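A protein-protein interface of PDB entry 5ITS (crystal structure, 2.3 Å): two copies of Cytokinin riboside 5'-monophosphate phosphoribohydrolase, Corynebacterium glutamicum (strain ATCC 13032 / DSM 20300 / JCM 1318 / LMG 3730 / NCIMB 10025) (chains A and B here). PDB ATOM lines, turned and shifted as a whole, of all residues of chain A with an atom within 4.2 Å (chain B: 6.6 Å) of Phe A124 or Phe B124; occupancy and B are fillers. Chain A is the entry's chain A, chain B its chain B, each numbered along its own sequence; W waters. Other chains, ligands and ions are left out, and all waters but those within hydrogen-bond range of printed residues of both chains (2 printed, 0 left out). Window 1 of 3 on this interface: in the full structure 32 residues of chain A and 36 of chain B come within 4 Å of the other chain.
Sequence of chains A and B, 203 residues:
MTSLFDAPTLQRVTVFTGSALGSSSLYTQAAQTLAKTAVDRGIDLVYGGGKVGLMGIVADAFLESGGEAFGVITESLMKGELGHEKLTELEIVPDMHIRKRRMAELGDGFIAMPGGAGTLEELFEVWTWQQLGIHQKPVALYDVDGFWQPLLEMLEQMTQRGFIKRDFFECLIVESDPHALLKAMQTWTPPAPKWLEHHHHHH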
ATOM      1  N   LEU A 120      20.168  19.644  20.760  1.00  0.00           N
ATOM      2  CA  LEU A 120      18.793  19.276  21.053  1.00  0.00           C
ATOM      3  C   LEU A 120      17.908  19.577  19.881  1.00  0.00           C
ATOM      4  O   LEU A 120      17.140  18.749  19.445  1.00  0.00           O
ATOM      5  CB  LEU A 120      18.300  20.000  22.272  1.00  0.00           C
ATOM      6  CG  LEU A 120      18.790  19.434  23.595  1.00  0.00           C
ATOM      7  CD1 LEU A 120      18.532  20.475  24.662  1.00  0.00           C
ATOM      8  CD2 LEU A 120      18.109  18.146  24.011  1.00  0.00           C
ATOM      9  N   GLU A 121      18.056  20.771  19.354  1.00  0.00           N
ATOM     10  CA  GLU A 121      17.276  21.289  18.232  1.00  0.00           C
ATOM     11  C   GLU A 121      17.393  20.397  17.008  1.00  0.00           C
ATOM     12  O   GLU A 121      16.424  20.074  16.406  1.00  0.00           O
ATOM     13  CB  GLU A 121      17.838  22.693  17.910  1.00  0.00           C
ATOM     14  CG  GLU A 121      17.246  23.395  16.708  1.00  0.00           C
ATOM     15  CD  GLU A 121      18.139  23.540  15.478  1.00  0.00           C
ATOM     16  OE1 GLU A 121      19.272  24.107  15.504  1.00  0.00           O
ATOM     17  OE2 GLU A 121      17.644  23.125  14.414  1.00  0.00           O
ATOM     18  N   GLU A 122      18.592  20.029  16.612  1.00  0.00           N
ATOM     19  CA  GLU A 122      18.786  19.128  15.456  1.00  0.00           C
ATOM     20  C   GLU A 122      18.198  17.722  15.681  1.00  0.00           C
ATOM     21  O   GLU A 122      17.555  17.155  14.799  1.00  0.00           O
ATOM     22  CB  GLU A 122      20.274  19.017  15.159  1.00  0.00           C
ATOM     23  CG  GLU A 122      20.825  20.343  14.658  1.00  0.00           C
ATOM     24  CD  GLU A 122      22.258  20.697  15.091  1.00  0.00           C
ATOM     25  OE1 GLU A 122      22.930  19.857  15.735  1.00  0.00           O
ATOM     26  OE2 GLU A 122      22.745  21.823  14.751  1.00  0.00           O
ATOM     27  N   LEU A 123      18.470  17.189  16.870  1.00  0.00           N
ATOM     28  CA  LEU A 123      18.003  15.905  17.348  1.00  0.00           C
ATOM     29  C   LEU A 123      16.492  15.840  17.242  1.00  0.00           C
ATOM     30  O   LEU A 123      15.959  14.957  16.593  1.00  0.00           O
ATOM     31  CB  LEU A 123      18.435  15.690  18.836  1.00  0.00           C
ATOM     32  CG  LEU A 123      17.731  14.509  19.501  1.00  0.00           C
ATOM     33  CD1 LEU A 123      17.953  13.218  18.728  1.00  0.00           C
ATOM     34  CD2 LEU A 123      18.121  14.312  20.928  1.00  0.00           C
ATOM     35  N   PHE A 124      15.808  16.793  17.863  1.00  0.00           N
ATOM     36  CA  PHE A 124      14.365  16.747  17.854  1.00  0.00           C
ATOM     37  C   PHE A 124      13.728  16.956  16.515  1.00  0.00           C
ATOM     38  O   PHE A 124      12.636  16.410  16.254  1.00  0.00           O
ATOM     39  CB  PHE A 124      13.755  17.598  18.960  1.00  0.00           C
ATOM     40  CG  PHE A 124      13.839  16.918  20.287  1.00  0.00           C
ATOM     41  CD1 PHE A 124      13.047  15.817  20.551  1.00  0.00           C
ATOM     42  CD2 PHE A 124      14.770  17.296  21.241  1.00  0.00           C
ATOM     43  CE1 PHE A 124      13.143  15.155  21.778  1.00  0.00           C
ATOM     44  CE2 PHE A 124      14.885  16.635  22.455  1.00  0.00           C
ATOM     45  CZ  PHE A 124      14.085  15.570  22.739  1.00  0.00           C
ATOM     46  N   GLU A 125      14.401  17.685  15.656  1.00  0.00           N
ATOM     47  CA  GLU A 125      13.853  17.860  14.369  1.00  0.00           C
ATOM     48  C   GLU A 125      13.875  16.522  13.717  1.00  0.00           C
ATOM     49  O   GLU A 125      12.838  16.097  13.268  1.00  0.00           O
ATOM     50  CB  GLU A 125      14.614  18.831  13.503  1.00  0.00           C
ATOM     51  CG  GLU A 125      14.103  18.856  12.045  1.00  0.00           C
ATOM     52  CD  GLU A 125      14.636  20.019  11.255  1.00  0.00           C
ATOM     53  OE1 GLU A 125      15.561  19.832  10.420  1.00  0.00           O
ATOM     54  OE2 GLU A 125      14.121  21.137  11.475  1.00  0.00           O
ATOM     55  N   VAL A 126      15.020  15.841  13.657  1.00  0.00           N
ATOM     56  CA  VAL A 126      15.049  14.612  12.841  1.00  0.00           C
ATOM     57  C   VAL A 126      14.246  13.483  13.489  1.00  0.00           C
ATOM     58  O   VAL A 126      13.801  12.554  12.779  1.00  0.00           O
ATOM     59  CB  VAL A 126      16.468  14.068  12.517  1.00  0.00           C
ATOM     60  CG1 VAL A 126      17.218  15.070  11.669  1.00  0.00           C
ATOM     61  CG2 VAL A 126      17.279  13.757  13.781  1.00  0.00           C
ATOM     62  N   TRP A 127      14.074  13.545  14.815  1.00  0.00           N
ATOM     63  CA  TRP A 127      13.297  12.512  15.501  1.00  0.00           C
ATOM     64  C   TRP A 127      11.854  12.722  15.156  1.00  0.00           C
ATOM     65  O   TRP A 127      11.186  11.815  14.783  1.00  0.00           O
ATOM     66  CB  TRP A 127      13.485  12.541  17.005  1.00  0.00           C
ATOM     67  CG  TRP A 127      13.012  11.316  17.673  1.00  0.00           C
ATOM     68  CD1 TRP A 127      13.179  10.016  17.253  1.00  0.00           C
ATOM     69  CD2 TRP A 127      12.344  11.238  18.936  1.00  0.00           C
ATOM     70  NE1 TRP A 127      12.620   9.154  18.154  1.00  0.00           N
ATOM     71  CE2 TRP A 127      12.111   9.874  19.200  1.00  0.00           C
ATOM     72  CE3 TRP A 127      11.862  12.187  19.823  1.00  0.00           C
ATOM     73  CZ2 TRP A 127      11.422   9.438  20.338  1.00  0.00           C
ATOM     74  CZ3 TRP A 127      11.213  11.769  20.971  1.00  0.00           C
ATOM     75  CH2 TRP A 127      10.996  10.396  21.221  1.00  0.00           C
ATOM     76  N   THR A 128      11.412  13.959  15.212  1.00  0.00           N
ATOM     77  CA  THR A 128      10.032  14.280  14.949  1.00  0.00           C
ATOM     78  C   THR A 128       9.679  13.906  13.550  1.00  0.00           C
ATOM     79  O   THR A 128       8.658  13.280  13.298  1.00  0.00           O
ATOM     80  CB  THR A 128       9.774  15.776  15.161  1.00  0.00           C
ATOM     81  OG1 THR A 128       9.943  16.113  16.562  1.00  0.00           O
ATOM     82  CG2 THR A 128       8.392  16.109  14.761  1.00  0.00           C
ATOM     83  N   LEU A 151      17.126  13.451  29.660  1.00  0.00           N
ATOM     84  CA  LEU A 151      16.303  13.574  28.513  1.00  0.00           C
ATOM     85  C   LEU A 151      15.344  12.410  28.412  1.00  0.00           C
ATOM     86  O   LEU A 151      14.194  12.605  28.050  1.00  0.00           O
ATOM     87  CB  LEU A 151      17.150  13.616  27.243  1.00  0.00           C
ATOM     88  CG  LEU A 151      16.293  13.696  25.965  1.00  0.00           C
ATOM     89  CD1 LEU A 151      15.923  15.146  25.900  1.00  0.00           C
ATOM     90  CD2 LEU A 151      16.923  13.360  24.624  1.00  0.00           C
ATOM     91  N   MET A 154      12.527  12.915  30.687  1.00  0.00           N
ATOM     92  CA  MET A 154      11.602  13.901  30.207  1.00  0.00           C
ATOM     93  C   MET A 154      10.717  13.245  29.177  1.00  0.00           C
ATOM     94  O   MET A 154       9.529  13.362  29.251  1.00  0.00           O
ATOM     95  CB  MET A 154      12.341  15.041  29.603  1.00  0.00           C
ATOM     96  CG  MET A 154      11.441  16.127  29.057  1.00  0.00           C
ATOM     97  SD  MET A 154      12.402  17.255  28.022  1.00  0.00           S
ATOM     98  CE  MET A 154      12.943  16.143  26.704  1.00  0.00           C
ATOM     99  N   LEU A 155      11.297  12.552  28.218  1.00  0.00           N
ATOM    100  CA  LEU A 155      10.485  11.860  27.247  1.00  0.00           C
ATOM    101  C   LEU A 155       9.550  10.811  27.899  1.00  0.00           C
ATOM    102  O   LEU A 155       8.403  10.605  27.468  1.00  0.00           O
ATOM    103  CB  LEU A 155      11.394  11.182  26.233  1.00  0.00           C
ATOM    104  CG  LEU A 155      12.185  12.180  25.377  1.00  0.00           C
ATOM    105  CD1 LEU A 155      12.890  11.440  24.268  1.00  0.00           C
ATOM    106  CD2 LEU A 155      11.305  13.252  24.784  1.00  0.00           C
ATOM    107  N   GLY B 116       4.502  17.220  22.635  1.00  0.00           N
ATOM    108  CA  GLY B 116       5.506  16.226  22.490  1.00  0.00           C
ATOM    109  C   GLY B 116       6.729  16.648  21.730  1.00  0.00           C
ATOM    110  O   GLY B 116       7.199  17.749  21.842  1.00  0.00           O
ATOM    111  N   ALA B 117       7.239  15.713  20.946  1.00  0.00           N
ATOM    112  CA  ALA B 117       8.455  15.879  20.164  1.00  0.00           C
ATOM    113  C   ALA B 117       8.477  17.141  19.332  1.00  0.00           C
ATOM    114  O   ALA B 117       9.475  17.904  19.356  1.00  0.00           O
ATOM    115  CB  ALA B 117       8.628  14.676  19.234  1.00  0.00           C
ATOM    116  N   GLY B 118       7.400  17.316  18.568  1.00  0.00           N
ATOM    117  CA  GLY B 118       7.276  18.462  17.684  1.00  0.00           C
ATOM    118  C   GLY B 118       7.370  19.770  18.448  1.00  0.00           C
ATOM    119  O   GLY B 118       7.965  20.741  17.983  1.00  0.00           O
ATOM    120  N   THR B 119       6.832  19.785  19.653  1.00  0.00           N
ATOM    121  CA  THR B 119       6.829  21.014  20.434  1.00  0.00           C
ATOM    122  C   THR B 119       8.267  21.309  20.830  1.00  0.00           C
ATOM    123  O   THR B 119       8.725  22.414  20.658  1.00  0.00           O
ATOM    124  CB  THR B 119       5.895  20.876  21.633  1.00  0.00           C
ATOM    125  OG1 THR B 119       4.542  20.782  21.168  1.00  0.00           O
ATOM    126  CG2 THR B 119       5.985  22.068  22.506  1.00  0.00           C
ATOM    127  N   LEU B 120       8.981  20.298  21.301  1.00  0.00           N
ATOM    128  CA  LEU B 120      10.430  20.356  21.541  1.00  0.00           C
ATOM    129  C   LEU B 120      11.227  20.731  20.311  1.00  0.00           C
ATOM    130  O   LEU B 120      12.088  21.530  20.420  1.00  0.00           O
ATOM    131  CB  LEU B 120      10.947  19.029  22.089  1.00  0.00           C
ATOM    132  CG  LEU B 120      10.434  18.581  23.491  1.00  0.00           C
ATOM    133  CD1 LEU B 120      10.969  17.222  23.841  1.00  0.00           C
ATOM    134  CD2 LEU B 120      10.829  19.556  24.610  1.00  0.00           C
ATOM    135  N   GLU B 121      10.946  20.183  19.135  1.00  0.00           N
ATOM    136  CA  GLU B 121      11.620  20.619  17.902  1.00  0.00           C
ATOM    137  C   GLU B 121      11.603  22.147  17.745  1.00  0.00           C
ATOM    138  O   GLU B 121      12.562  22.755  17.311  1.00  0.00           O
ATOM    139  CB  GLU B 121      10.890  20.012  16.694  1.00  0.00           C
ATOM    140  CG  GLU B 121      11.224  20.591  15.333  1.00  0.00           C
ATOM    141  CD  GLU B 121      10.430  19.934  14.213  1.00  0.00           C
ATOM    142  OE1 GLU B 121      10.708  20.205  13.003  1.00  0.00           O
ATOM    143  OE2 GLU B 121       9.524  19.129  14.545  1.00  0.00           O
ATOM    144  N   GLU B 122      10.460  22.739  18.036  1.00  0.00           N
ATOM    145  CA  GLU B 122      10.188  24.150  17.771  1.00  0.00           C
ATOM    146  C   GLU B 122      10.799  25.033  18.847  1.00  0.00           C
ATOM    147  O   GLU B 122      11.469  26.031  18.543  1.00  0.00           O
ATOM    148  CB  GLU B 122       8.675  24.365  17.685  1.00  0.00           C
ATOM    149  CG  GLU B 122       8.096  23.782  16.403  1.00  0.00           C
ATOM    150  CD  GLU B 122       6.577  23.517  16.418  1.00  0.00           C
ATOM    151  OE1 GLU B 122       5.898  23.549  17.507  1.00  0.00           O
ATOM    152  OE2 GLU B 122       6.052  23.260  15.281  1.00  0.00           O
ATOM    153  N   LEU B 123      10.568  24.640  20.089  1.00  0.00           N
ATOM    154  CA  LEU B 123      11.126  25.332  21.243  1.00  0.00           C
ATOM    155  C   LEU B 123      12.638  25.457  21.170  1.00  0.00           C
ATOM    156  O   LEU B 123      13.187  26.512  21.232  1.00  0.00           O
ATOM    157  CB  LEU B 123      10.775  24.549  22.487  1.00  0.00           C
ATOM    158  CG  LEU B 123      11.436  25.052  23.763  1.00  0.00           C
ATOM    159  CD1 LEU B 123      11.125  26.513  23.980  1.00  0.00           C
ATOM    160  CD2 LEU B 123      10.936  24.257  24.973  1.00  0.00           C
ATOM    161  N   PHE B 124      13.331  24.353  21.042  1.00  0.00           N
ATOM    162  CA  PHE B 124      14.782  24.408  20.981  1.00  0.00           C
ATOM    163  C   PHE B 124      15.320  25.152  19.794  1.00  0.00           C
ATOM    164  O   PHE B 124      16.418  25.710  19.881  1.00  0.00           O
ATOM    165  CB  PHE B 124      15.378  22.984  21.037  1.00  0.00           C
ATOM    166  CG  PHE B 124      15.138  22.326  22.332  1.00  0.00           C
ATOM    167  CD1 PHE B 124      15.395  23.014  23.515  1.00  0.00           C
ATOM    168  CD2 PHE B 124      14.617  21.059  22.397  1.00  0.00           C
ATOM    169  CE1 PHE B 124      15.140  22.447  24.744  1.00  0.00           C
ATOM    170  CE2 PHE B 124      14.399  20.484  23.619  1.00  0.00           C
ATOM    171  CZ  PHE B 124      14.663  21.192  24.794  1.00  0.00           C
ATOM    172  N   GLU B 125      14.596  25.151  18.688  1.00  0.00           N
ATOM    173  CA  GLU B 125      15.073  25.890  17.563  1.00  0.00           C
ATOM    174  C   GLU B 125      15.065  27.387  17.846  1.00  0.00           C
ATOM    175  O   GLU B 125      16.045  28.043  17.727  1.00  0.00           O
ATOM    176  CB  GLU B 125      14.286  25.599  16.321  1.00  0.00           C
ATOM    177  CG  GLU B 125      14.960  26.255  15.127  1.00  0.00           C
ATOM    178  CD  GLU B 125      14.381  25.813  13.783  1.00  0.00           C
ATOM    179  OE1 GLU B 125      13.150  25.883  13.668  1.00  0.00           O
ATOM    180  OE2 GLU B 125      15.149  25.425  12.861  1.00  0.00           O
ATOM    181  N   VAL B 126      13.943  27.902  18.274  1.00  0.00           N
ATOM    182  CA  VAL B 126      13.831  29.323  18.549  1.00  0.00           C
ATOM    183  C   VAL B 126      14.723  29.770  19.711  1.00  0.00           C
ATOM    184  O   VAL B 126      15.176  30.894  19.709  1.00  0.00           O
ATOM    185  CB  VAL B 126      12.368  29.792  18.811  1.00  0.00           C
ATOM    186  CG1 VAL B 126      11.478  29.508  17.613  1.00  0.00           C
ATOM    187  CG2 VAL B 126      11.804  29.177  20.061  1.00  0.00           C
ATOM    188  N   TRP B 127      14.948  28.907  20.682  1.00  0.00           N
ATOM    189  CA  TRP B 127      15.855  29.220  21.761  1.00  0.00           C
ATOM    190  C   TRP B 127      17.301  29.260  21.229  1.00  0.00           C
ATOM    191  O   TRP B 127      18.112  30.140  21.599  1.00  0.00           O
ATOM    192  CB  TRP B 127      15.756  28.154  22.833  1.00  0.00           C
ATOM    193  CG  TRP B 127      16.363  28.550  24.102  1.00  0.00           C
ATOM    194  CD1 TRP B 127      16.302  29.754  24.646  1.00  0.00           C
ATOM    195  CD2 TRP B 127      17.065  27.721  25.029  1.00  0.00           C
ATOM    196  NE1 TRP B 127      16.930  29.771  25.862  1.00  0.00           N
ATOM    197  CE2 TRP B 127      17.417  28.535  26.125  1.00  0.00           C
ATOM    198  CE3 TRP B 127      17.450  26.383  25.037  1.00  0.00           C
ATOM    199  CZ2 TRP B 127      18.132  28.073  27.223  1.00  0.00           C
ATOM    200  CZ3 TRP B 127      18.170  25.904  26.145  1.00  0.00           C
ATOM    201  CH2 TRP B 127      18.504  26.757  27.214  1.00  0.00           C
ATOM    202  N   THR B 128      17.637  28.298  20.368  1.00  0.00           N
ATOM    203  CA  THR B 128      18.982  28.296  19.778  1.00  0.00           C
ATOM    204  C   THR B 128      19.188  29.592  19.034  1.00  0.00           C
ATOM    205  O   THR B 128      20.212  30.244  19.167  1.00  0.00           O
ATOM    206  CB  THR B 128      19.205  27.074  18.887  1.00  0.00           C
ATOM    207  OG1 THR B 128      19.109  25.937  19.721  1.00  0.00           O
ATOM    208  CG2 THR B 128      20.558  27.027  18.344  1.00  0.00           C
ATOM    209  N   TRP B 129      18.179  29.976  18.272  1.00  0.00           N
ATOM    210  CA  TRP B 129      18.274  31.182  17.478  1.00  0.00           C
ATOM    211  C   TRP B 129      18.444  32.471  18.302  1.00  0.00           C
ATOM    212  O   TRP B 129      19.123  33.391  17.872  1.00  0.00           O
ATOM    213  CB  TRP B 129      17.055  31.302  16.606  1.00  0.00           C
ATOM    214  CG  TRP B 129      17.013  30.348  15.532  1.00  0.00           C
ATOM    215  CD1 TRP B 129      17.988  29.508  15.118  1.00  0.00           C
ATOM    216  CD2 TRP B 129      15.919  30.136  14.679  1.00  0.00           C
ATOM    217  NE1 TRP B 129      17.566  28.765  14.035  1.00  0.00           N
ATOM    218  CE2 TRP B 129      16.290  29.147  13.749  1.00  0.00           C
ATOM    219  CE3 TRP B 129      14.657  30.697  14.598  1.00  0.00           C
ATOM    220  CZ2 TRP B 129      15.454  28.727  12.769  1.00  0.00           C
ATOM    221  CZ3 TRP B 129      13.816  30.263  13.637  1.00  0.00           C
ATOM    222  CH2 TRP B 129      14.205  29.293  12.728  1.00  0.00           C
ATOM    223  N   LEU B 151      12.253  18.813  31.838  1.00  0.00           N
ATOM    224  CA  LEU B 151      13.068  19.535  30.863  1.00  0.00           C
ATOM    225  C   LEU B 151      14.049  20.460  31.589  1.00  0.00           C
ATOM    226  O   LEU B 151      15.223  20.514  31.254  1.00  0.00           O
ATOM    227  CB  LEU B 151      12.166  20.339  29.943  1.00  0.00           C
ATOM    228  CG  LEU B 151      12.782  21.001  28.733  1.00  0.00           C
ATOM    229  CD1 LEU B 151      11.746  21.138  27.648  1.00  0.00           C
ATOM    230  CD2 LEU B 151      13.248  22.394  29.050  1.00  0.00           C
ATOM    231  N   MET B 154      16.824  18.593  32.906  1.00  0.00           N
ATOM    232  CA  MET B 154      17.734  18.248  31.814  1.00  0.00           C
ATOM    233  C   MET B 154      18.615  19.400  31.390  1.00  0.00           C
ATOM    234  O   MET B 154      19.798  19.202  31.205  1.00  0.00           O
ATOM    235  CB  MET B 154      17.011  17.750  30.584  1.00  0.00           C
ATOM    236  CG  MET B 154      17.896  17.732  29.355  1.00  0.00           C
ATOM    237  SD  MET B 154      17.029  17.306  27.826  1.00  0.00           S
ATOM    238  CE  MET B 154      16.222  18.843  27.466  1.00  0.00           C
ATOM    239  N   LEU B 155      18.062  20.591  31.231  1.00  0.00           N
ATOM    240  CA  LEU B 155      18.877  21.723  30.901  1.00  0.00           C
ATOM    241  C   LEU B 155      19.847  22.110  32.042  1.00  0.00           C
ATOM    242  O   LEU B 155      20.954  22.581  31.790  1.00  0.00           O
ATOM    243  CB  LEU B 155      18.006  22.893  30.548  1.00  0.00           C
ATOM    244  CG  LEU B 155      17.172  22.685  29.282  1.00  0.00           C
ATOM    245  CD1 LEU B 155      16.334  23.936  29.043  1.00  0.00           C
ATOM    246  CD2 LEU B 155      17.989  22.374  28.037  1.00  0.00           C
HETATM  247  O   HOH W   1      17.869  25.808  13.115  1.00  0.00           O
HETATM  248  O   HOH W   2      14.228  22.058  15.022  1.00  0.00           O
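OG1 of Thr A128 sits close to O of Ala B117 (3.4 Å). The side-chain hydroxyl (OG1) of Thr A128 is in hydrogen-bond range of the backbone NH (N) of Gly B118.
The side-chain hydroxyl of Thr A128 lies within hydrogen-bond range of the backbone carbonyl oxygen of Phe A124 (2.7 Å). OG1 of Thr B128 sits at hydrogen-bond distance from O of Phe B124, at 2.7 Å.
CD2 of Phe B124 touches CB of Leu A120 (3.8 Å). Met B154 touches Leu A120 (CE to CD1, 3.98 Å). Glu A121 touches Phe B124 (CA to CB, 3.8 Å). Glu A121 touches Thr B128. Phe A124 touches Leu B120 (CE1 to CD1, 3.6 Å). Glu B121 touches Phe A124 (N to CB, 3.8 Å). CD2 of Phe A124 touches CD2 of Phe B124 (3.9 Å). Glu A125 touches Glu B121. Thr A128 touches Glu B121. Met A154 touches Leu B120.
Phe A124 touches just these residues of chain B: Leu B120, Glu B121 and Phe B124. Of the printed residues of chain A, Phe B124 touches Leu A120, Glu A121 and Phe A124. Of the printed residues of chain B, Glu A125 touches Glu B121 (3.8 Å). Printed residues of chain B within 4 Å of Met A154: Leu B120 (3.6 Å) and Leu B151 (3.6 Å). The nearest residue of chain B that does not touch Phe A124 is Ala B117 (4.3 Å).
Among the printed residues, 16 pairs touch across the chains. Among the printed residues, no Asp or Glu carboxylate lies within 4 Å of a Lys or Arg side-chain nitrogen of the other chain.
Leu A120 touches Met B154, and with the chains exchanged Met A154 touches Leu B120. Leu A120 touches Leu B155, but with the chains exchanged Leu A155 does not touch Leu B120 (4.1 Å). Glu A121 touches Glu B125, and with the chains exchanged Glu A125 touches Glu B121. Leu A151 touches Met B154, and with the chains exchanged Met A154 touches Leu B151. Of the 16 pairs that touch across the chains among the printed residues, 13 have their exchanged pair printed and touching as well.
Water W1 lies within hydrogen-bond range of OE2 of Glu B125 (2.8 Å), OE2 of Glu A121 (3.0 Å) and NE1 of Trp B129 (3.1 Å). Water W2 bridges the backbone carbonyl oxygen of Glu B121 and the backbone carbonyl oxygen of Glu A121.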
